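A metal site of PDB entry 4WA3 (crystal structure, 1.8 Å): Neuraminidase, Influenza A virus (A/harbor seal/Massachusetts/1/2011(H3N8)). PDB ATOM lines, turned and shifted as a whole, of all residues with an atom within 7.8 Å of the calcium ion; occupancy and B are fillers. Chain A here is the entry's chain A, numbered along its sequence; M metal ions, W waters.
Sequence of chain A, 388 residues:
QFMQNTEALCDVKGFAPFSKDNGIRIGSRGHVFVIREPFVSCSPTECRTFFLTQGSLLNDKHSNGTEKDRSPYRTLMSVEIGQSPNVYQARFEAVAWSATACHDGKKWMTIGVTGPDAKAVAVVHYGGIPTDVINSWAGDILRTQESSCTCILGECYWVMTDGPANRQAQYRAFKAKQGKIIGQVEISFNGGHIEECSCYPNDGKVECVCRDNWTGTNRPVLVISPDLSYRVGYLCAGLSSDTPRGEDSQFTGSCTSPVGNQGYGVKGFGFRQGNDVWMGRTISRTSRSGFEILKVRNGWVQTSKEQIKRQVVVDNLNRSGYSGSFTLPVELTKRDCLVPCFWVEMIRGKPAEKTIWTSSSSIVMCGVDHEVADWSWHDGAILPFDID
Water W1 bridges O of Pro 244 (2.8 Å) and O of Gly 263 (3.0 Å).
The backbone NH of Gly 216 lies within hydrogen-bond range of the side-chain carboxylate of Asp 212.
The side-chain carboxylate (OD1) of Asp 242 is in salt-bridge range of the guanidinium group (NH1) of Arg 219 (3.8 Å).
The side-chain carboxylate (OD1) of Asp 212 lies within hydrogen-bond range of the backbone NH (N) of Trp 214, 2.7 Å away.
O of Thr 243 sits close to N of Gly 265 (3.5 Å).
The side-chain carboxylate (OD1) of Asp 242 is in hydrogen-bond range of the backbone NH (N) of Val 266 (2.8 Å).
The guanidinium group (NH1) of Arg 245 lies within hydrogen-bond range of the backbone carbonyl oxygen (O) of Asp 242 (3.1 Å).
O of Asn 213 sits at hydrogen-bond distance from N of Tyr 264, 3.4 Å away.
The guanidinium group (NH2) of Arg 211 sits at hydrogen-bond distance from the backbone carbonyl oxygen (O) of Gly 265 (3.2 Å).
Residues that only touch the calcium ion: Gly 265 (3.9 Å).
Within 4 Å of the calcium ion: Asp 212, Gly 216, Asp 242, Tyr 264 and Gly 265.
The nearest printed residue that does not touch the calcium ion is Gln 262 (4.1 Å).
The calcium ion is bound by O of Asp 212, at 2.3 Å.
The backbone carbonyl oxygen (O) of Tyr 264 binds the calcium ion, 2.3 Å away.
The calcium ion is bound by O of Gly 216 (2.3 Å).
The calcium ion is bound by the side-chain carboxylate (OD2) of Asp 242, at 2.4 Å.
Water W1 is bound to the calcium ion, at 2.4 Å.
Water W2 is bound to the calcium ion, at 2.5 Å.
The calcium ion has six donor atoms within binding distance.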
ATOM      1  N   HIS A 193     -25.081   1.946  25.681  1.00  0.00           N
ATOM      2  CA  HIS A 193     -25.052   0.494  25.851  1.00  0.00           C
ATOM      3  C   HIS A 193     -23.872   0.111  26.725  1.00  0.00           C
ATOM      4  O   HIS A 193     -22.761   0.609  26.527  1.00  0.00           O
ATOM      5  CB  HIS A 193     -24.966  -0.178  24.479  1.00  0.00           C
ATOM      6  CG  HIS A 193     -25.328  -1.632  24.495  1.00  0.00           C
ATOM      7  ND1 HIS A 193     -24.380  -2.628  24.501  1.00  0.00           N
ATOM      8  CD2 HIS A 193     -26.529  -2.253  24.504  1.00  0.00           C
ATOM      9  CE1 HIS A 193     -24.979  -3.809  24.501  1.00  0.00           C
ATOM     10  NE2 HIS A 193     -26.284  -3.601  24.508  1.00  0.00           N
ATOM     11  N   ARG A 211     -18.106  -1.650  27.760  1.00  0.00           N
ATOM     12  CA  ARG A 211     -18.195  -1.860  26.323  1.00  0.00           C
ATOM     13  C   ARG A 211     -19.578  -1.493  25.829  1.00  0.00           C
ATOM     14  O   ARG A 211     -20.574  -1.984  26.344  1.00  0.00           O
ATOM     15  CB  ARG A 211     -17.892  -3.325  26.008  1.00  0.00           C
ATOM     16  CG  ARG A 211     -18.228  -3.782  24.594  1.00  0.00           C
ATOM     17  CD  ARG A 211     -18.006  -5.265  24.498  1.00  0.00           C
ATOM     18  NE  ARG A 211     -18.456  -5.869  23.255  1.00  0.00           N
ATOM     19  CZ  ARG A 211     -18.241  -7.140  22.926  1.00  0.00           C
ATOM     20  NH1 ARG A 211     -17.570  -7.939  23.739  1.00  0.00           N
ATOM     21  NH2 ARG A 211     -18.697  -7.616  21.774  1.00  0.00           N
ATOM     22  N   ASP A 212     -19.607  -0.618  24.819  1.00  0.00           N
ATOM     23  CA  ASP A 212     -20.810  -0.274  24.087  1.00  0.00           C
ATOM     24  C   ASP A 212     -20.838  -1.101  22.822  1.00  0.00           C
ATOM     25  O   ASP A 212     -19.971  -0.969  21.967  1.00  0.00           O
ATOM     26  CB  ASP A 212     -20.807   1.229  23.735  1.00  0.00           C
ATOM     27  CG  ASP A 212     -22.056   1.666  22.976  1.00  0.00           C
ATOM     28  OD1 ASP A 212     -22.526   0.947  22.072  1.00  0.00           O
ATOM     29  OD2 ASP A 212     -22.560   2.773  23.262  1.00  0.00           O
ATOM     30  N   ASN A 213     -21.826  -1.978  22.703  1.00  0.00           N
ATOM     31  CA  ASN A 213     -21.928  -2.887  21.577  1.00  0.00           C
ATOM     32  C   ASN A 213     -22.990  -2.441  20.576  1.00  0.00           C
ATOM     33  O   ASN A 213     -23.306  -3.163  19.625  1.00  0.00           O
ATOM     34  CB  ASN A 213     -22.267  -4.285  22.095  1.00  0.00           C
ATOM     35  CG  ASN A 213     -21.626  -5.369  21.264  1.00  0.00           C
ATOM     36  OD1 ASN A 213     -20.399  -5.439  21.160  1.00  0.00           O
ATOM     37  ND2 ASN A 213     -22.452  -6.238  20.677  1.00  0.00           N
ATOM     38  N   TRP A 214     -23.533  -1.246  20.781  1.00  0.00           N
ATOM     39  CA  TRP A 214     -24.643  -0.716  19.993  1.00  0.00           C
ATOM     40  C   TRP A 214     -24.151   0.245  18.897  1.00  0.00           C
ATOM     41  O   TRP A 214     -24.096  -0.138  17.736  1.00  0.00           O
ATOM     42  CB  TRP A 214     -25.633  -0.038  20.934  1.00  0.00           C
ATOM     43  CG  TRP A 214     -26.882   0.503  20.313  1.00  0.00           C
ATOM     44  CD1 TRP A 214     -27.282   0.397  19.009  1.00  0.00           C
ATOM     45  CD2 TRP A 214     -27.904   1.252  20.980  1.00  0.00           C
ATOM     46  NE1 TRP A 214     -28.478   1.033  18.825  1.00  0.00           N
ATOM     47  CE2 TRP A 214     -28.889   1.569  20.026  1.00  0.00           C
ATOM     48  CE3 TRP A 214     -28.078   1.678  22.293  1.00  0.00           C
ATOM     49  CZ2 TRP A 214     -30.036   2.288  20.342  1.00  0.00           C
ATOM     50  CZ3 TRP A 214     -29.216   2.399  22.620  1.00  0.00           C
ATOM     51  CH2 TRP A 214     -30.180   2.699  21.643  1.00  0.00           C
ATOM     52  N   THR A 215     -23.808   1.478  19.263  1.00  0.00           N
ATOM     53  CA  THR A 215     -23.310   2.464  18.290  1.00  0.00           C
ATOM     54  C   THR A 215     -21.947   3.094  18.633  1.00  0.00           C
ATOM     55  O   THR A 215     -21.343   3.783  17.806  1.00  0.00           O
ATOM     56  CB  THR A 215     -24.305   3.647  18.073  1.00  0.00           C
ATOM     57  OG1 THR A 215     -24.332   4.478  19.243  1.00  0.00           O
ATOM     58  CG2 THR A 215     -25.711   3.136  17.779  1.00  0.00           C
ATOM     59  N   GLY A 216     -21.451   2.868  19.841  1.00  0.00           N
ATOM     60  CA  GLY A 216     -20.295   3.610  20.330  1.00  0.00           C
ATOM     61  C   GLY A 216     -18.942   2.969  20.064  1.00  0.00           C
ATOM     62  O   GLY A 216     -18.766   1.767  20.248  1.00  0.00           O
ATOM     63  N   THR A 217     -17.971   3.772  19.624  1.00  0.00           N
ATOM     64  CA  THR A 217     -16.582   3.321  19.531  1.00  0.00           C
ATOM     65  C   THR A 217     -15.757   3.875  20.695  1.00  0.00           C
ATOM     66  O   THR A 217     -14.589   3.515  20.860  1.00  0.00           O
ATOM     67  CB  THR A 217     -15.923   3.749  18.211  1.00  0.00           C
ATOM     68  OG1 THR A 217     -15.764   5.167  18.180  1.00  0.00           O
ATOM     69  CG2 THR A 217     -16.754   3.284  17.012  1.00  0.00           C
ATOM     70  N   ASN A 218     -16.377   4.748  21.488  1.00  0.00           N
ATOM     71  CA  ASN A 218     -15.811   5.161  22.767  1.00  0.00           C
ATOM     72  C   ASN A 218     -16.455   4.320  23.872  1.00  0.00           C
ATOM     73  O   ASN A 218     -17.504   3.710  23.670  1.00  0.00           O
ATOM     74  CB  ASN A 218     -16.033   6.659  23.013  1.00  0.00           C
ATOM     75  CG  ASN A 218     -17.457   7.109  22.756  1.00  0.00           C
ATOM     76  OD1 ASN A 218     -18.198   6.485  21.992  1.00  0.00           O
ATOM     77  ND2 ASN A 218     -17.852   8.210  23.376  1.00  0.00           N
ATOM     78  N   ARG A 219     -15.818   4.270  25.032  1.00  0.00           N
ATOM     79  CA  ARG A 219     -16.270   3.378  26.105  1.00  0.00           C
ATOM     80  C   ARG A 219     -17.115   4.087  27.150  1.00  0.00           C
ATOM     81  O   ARG A 219     -16.781   5.192  27.581  1.00  0.00           O
ATOM     82  CB  ARG A 219     -15.073   2.747  26.792  1.00  0.00           C
ATOM     83  CG  ARG A 219     -14.324   1.778  25.909  1.00  0.00           C
ATOM     84  CD  ARG A 219     -13.316   0.973  26.686  1.00  0.00           C
ATOM     85  NE  ARG A 219     -12.639   0.020  25.814  1.00  0.00           N
ATOM     86  CZ  ARG A 219     -13.193  -1.105  25.371  1.00  0.00           C
ATOM     87  NH1 ARG A 219     -12.493  -1.900  24.576  1.00  0.00           N
ATOM     88  NH2 ARG A 219     -14.432  -1.425  25.708  1.00  0.00           N
ATOM     89  N   PRO A 220     -18.230   3.454  27.563  1.00  0.00           N
ATOM     90  CA  PRO A 220     -18.972   3.991  28.701  1.00  0.00           C
ATOM     91  C   PRO A 220     -18.134   4.032  29.959  1.00  0.00           C
ATOM     92  O   PRO A 220     -17.226   3.213  30.132  1.00  0.00           O
ATOM     93  CB  PRO A 220     -20.119   2.994  28.871  1.00  0.00           C
ATOM     94  CG  PRO A 220     -20.337   2.458  27.515  1.00  0.00           C
ATOM     95  CD  PRO A 220     -18.967   2.368  26.900  1.00  0.00           C
ATOM     96  N   ASP A 242     -12.419   1.280  21.764  1.00  0.00           N
ATOM     97  CA  ASP A 242     -13.159   0.062  21.438  1.00  0.00           C
ATOM     98  C   ASP A 242     -12.576  -0.511  20.153  1.00  0.00           C
ATOM     99  O   ASP A 242     -11.764   0.120  19.501  1.00  0.00           O
ATOM    100  CB  ASP A 242     -14.655   0.344  21.263  1.00  0.00           C
ATOM    101  CG  ASP A 242     -15.515  -0.884  21.521  1.00  0.00           C
ATOM    102  OD1 ASP A 242     -14.948  -1.982  21.739  1.00  0.00           O
ATOM    103  OD2 ASP A 242     -16.771  -0.769  21.488  1.00  0.00           O
ATOM    104  N   THR A 243     -13.000  -1.717  19.814  1.00  0.00           N
ATOM    105  CA  THR A 243     -12.661  -2.346  18.545  1.00  0.00           C
ATOM    106  C   THR A 243     -13.905  -3.101  18.070  1.00  0.00           C
ATOM    107  O   THR A 243     -14.408  -3.963  18.799  1.00  0.00           O
ATOM    108  CB  THR A 243     -11.500  -3.341  18.708  1.00  0.00           C
ATOM    109  OG1 THR A 243     -10.407  -2.702  19.370  1.00  0.00           O
ATOM    110  CG2 THR A 243     -11.038  -3.854  17.352  1.00  0.00           C
ATOM    111  N   PRO A 244     -14.396  -2.808  16.861  1.00  0.00           N
ATOM    112  CA  PRO A 244     -13.903  -1.880  15.839  1.00  0.00           C
ATOM    113  C   PRO A 244     -14.084  -0.401  16.187  1.00  0.00           C
ATOM    114  O   PRO A 244     -14.968  -0.028  16.952  1.00  0.00           O
ATOM    115  CB  PRO A 244     -14.723  -2.241  14.599  1.00  0.00           C
ATOM    116  CG  PRO A 244     -15.968  -2.856  15.131  1.00  0.00           C
ATOM    117  CD  PRO A 244     -15.529  -3.605  16.345  1.00  0.00           C
ATOM    118  N   ARG A 245     -13.220   0.423  15.607  1.00  0.00           N
ATOM    119  CA  ARG A 245     -13.310   1.875  15.749  1.00  0.00           C
ATOM    120  C   ARG A 245     -12.797   2.523  14.477  1.00  0.00           C
ATOM    121  O   ARG A 245     -12.321   1.844  13.567  1.00  0.00           O
ATOM    122  CB  ARG A 245     -12.497   2.358  16.949  1.00  0.00           C
ATOM    123  CG  ARG A 245     -11.033   1.949  16.894  1.00  0.00           C
ATOM    124  CD  ARG A 245     -10.233   2.555  18.031  1.00  0.00           C
ATOM    125  NE  ARG A 245      -8.800   2.321  17.841  1.00  0.00           N
ATOM    126  CZ  ARG A 245      -8.177   1.183  18.105  1.00  0.00           C
ATOM    127  NH1 ARG A 245      -8.835   0.145  18.591  1.00  0.00           N
ATOM    128  NH2 ARG A 245      -6.883   1.086  17.873  1.00  0.00           N
ATOM    129  N   VAL A 259     -19.921   7.892  20.208  1.00  0.00           N
ATOM    130  CA  VAL A 259     -19.376   8.486  18.988  1.00  0.00           C
ATOM    131  C   VAL A 259     -18.831   7.388  18.092  1.00  0.00           C
ATOM    132  O   VAL A 259     -18.273   6.408  18.588  1.00  0.00           O
ATOM    133  CB  VAL A 259     -18.199   9.432  19.317  1.00  0.00           C
ATOM    134  CG1 VAL A 259     -17.790  10.249  18.089  1.00  0.00           C
ATOM    135  CG2 VAL A 259     -18.547  10.358  20.479  1.00  0.00           C
ATOM    136  N   ASN A 261     -20.559   5.750  15.323  1.00  0.00           N
ATOM    137  CA  ASN A 261     -21.583   4.996  14.589  1.00  0.00           C
ATOM    138  C   ASN A 261     -21.106   3.637  14.059  1.00  0.00           C
ATOM    139  O   ASN A 261     -21.198   3.364  12.867  1.00  0.00           O
ATOM    140  CB  ASN A 261     -22.116   5.816  13.412  1.00  0.00           C
ATOM    141  CG  ASN A 261     -22.518   7.224  13.807  1.00  0.00           C
ATOM    142  OD1 ASN A 261     -22.073   8.201  13.207  1.00  0.00           O
ATOM    143  ND2 ASN A 261     -23.351   7.329  14.835  1.00  0.00           N
ATOM    144  N   GLN A 262     -20.602   2.805  14.960  1.00  0.00           N
ATOM    145  CA  GLN A 262     -20.232   1.435  14.621  1.00  0.00           C
ATOM    146  C   GLN A 262     -20.758   0.469  15.662  1.00  0.00           C
ATOM    147  O   GLN A 262     -20.848   0.805  16.846  1.00  0.00           O
ATOM    148  CB  GLN A 262     -18.715   1.296  14.489  1.00  0.00           C
ATOM    149  CG  GLN A 262     -18.212   1.467  13.067  1.00  0.00           C
ATOM    150  CD  GLN A 262     -16.711   1.371  12.967  1.00  0.00           C
ATOM    151  OE1 GLN A 262     -15.997   2.364  13.148  1.00  0.00           O
ATOM    152  NE2 GLN A 262     -16.211   0.183  12.655  1.00  0.00           N
ATOM    153  N   GLY A 263     -21.095  -0.742  15.229  1.00  0.00           N
ATOM    154  CA  GLY A 263     -21.561  -1.770  16.135  1.00  0.00           C
ATOM    155  C   GLY A 263     -20.410  -2.603  16.642  1.00  0.00           C
ATOM    156  O   GLY A 263     -19.239  -2.351  16.314  1.00  0.00           O
ATOM    157  N   TYR A 264     -20.749  -3.608  17.441  1.00  0.00           N
ATOM    158  CA  TYR A 264     -19.801  -4.552  18.017  1.00  0.00           C
ATOM    159  C   TYR A 264     -18.842  -3.869  18.987  1.00  0.00           C
ATOM    160  O   TYR A 264     -19.081  -2.727  19.415  1.00  0.00           O
ATOM    161  CB  TYR A 264     -19.059  -5.333  16.925  1.00  0.00           C
ATOM    162  CG  TYR A 264     -18.556  -6.699  17.356  1.00  0.00           C
ATOM    163  CD1 TYR A 264     -19.360  -7.553  18.100  1.00  0.00           C
ATOM    164  CD2 TYR A 264     -17.278  -7.134  17.014  1.00  0.00           C
ATOM    165  CE1 TYR A 264     -18.897  -8.794  18.499  1.00  0.00           C
ATOM    166  CE2 TYR A 264     -16.822  -8.365  17.408  1.00  0.00           C
ATOM    167  CZ  TYR A 264     -17.631  -9.195  18.150  1.00  0.00           C
ATOM    168  OH  TYR A 264     -17.177 -10.439  18.539  1.00  0.00           O
ATOM    169  N   GLY A 265     -17.770  -4.545  19.365  1.00  0.00           N
ATOM    170  CA  GLY A 265     -16.923  -4.064  20.420  1.00  0.00           C
ATOM    171  C   GLY A 265     -16.050  -5.161  20.992  1.00  0.00           C
ATOM    172  O   GLY A 265     -16.067  -6.309  20.532  1.00  0.00           O
ATOM    173  N   VAL A 266     -15.284  -4.789  22.010  1.00  0.00           N
ATOM    174  CA  VAL A 266     -14.467  -5.747  22.732  1.00  0.00           C
ATOM    175  C   VAL A 266     -14.419  -5.258  24.171  1.00  0.00           C
ATOM    176  O   VAL A 266     -14.469  -4.055  24.419  1.00  0.00           O
ATOM    177  CB  VAL A 266     -13.040  -5.846  22.135  1.00  0.00           C
ATOM    178  CG1 VAL A 266     -12.249  -4.550  22.323  1.00  0.00           C
ATOM    179  CG2 VAL A 266     -12.288  -7.045  22.730  1.00  0.00           C
HETATM  180 CA    CA M   1     -18.697  -0.556  20.112  1.00  0.00          CA
HETATM  181  O   HOH W   1     -17.508  -0.651  18.018  1.00  0.00           O
HETATM  182  O   HOH W   2     -20.901  -0.252  18.979  1.00  0.00           O
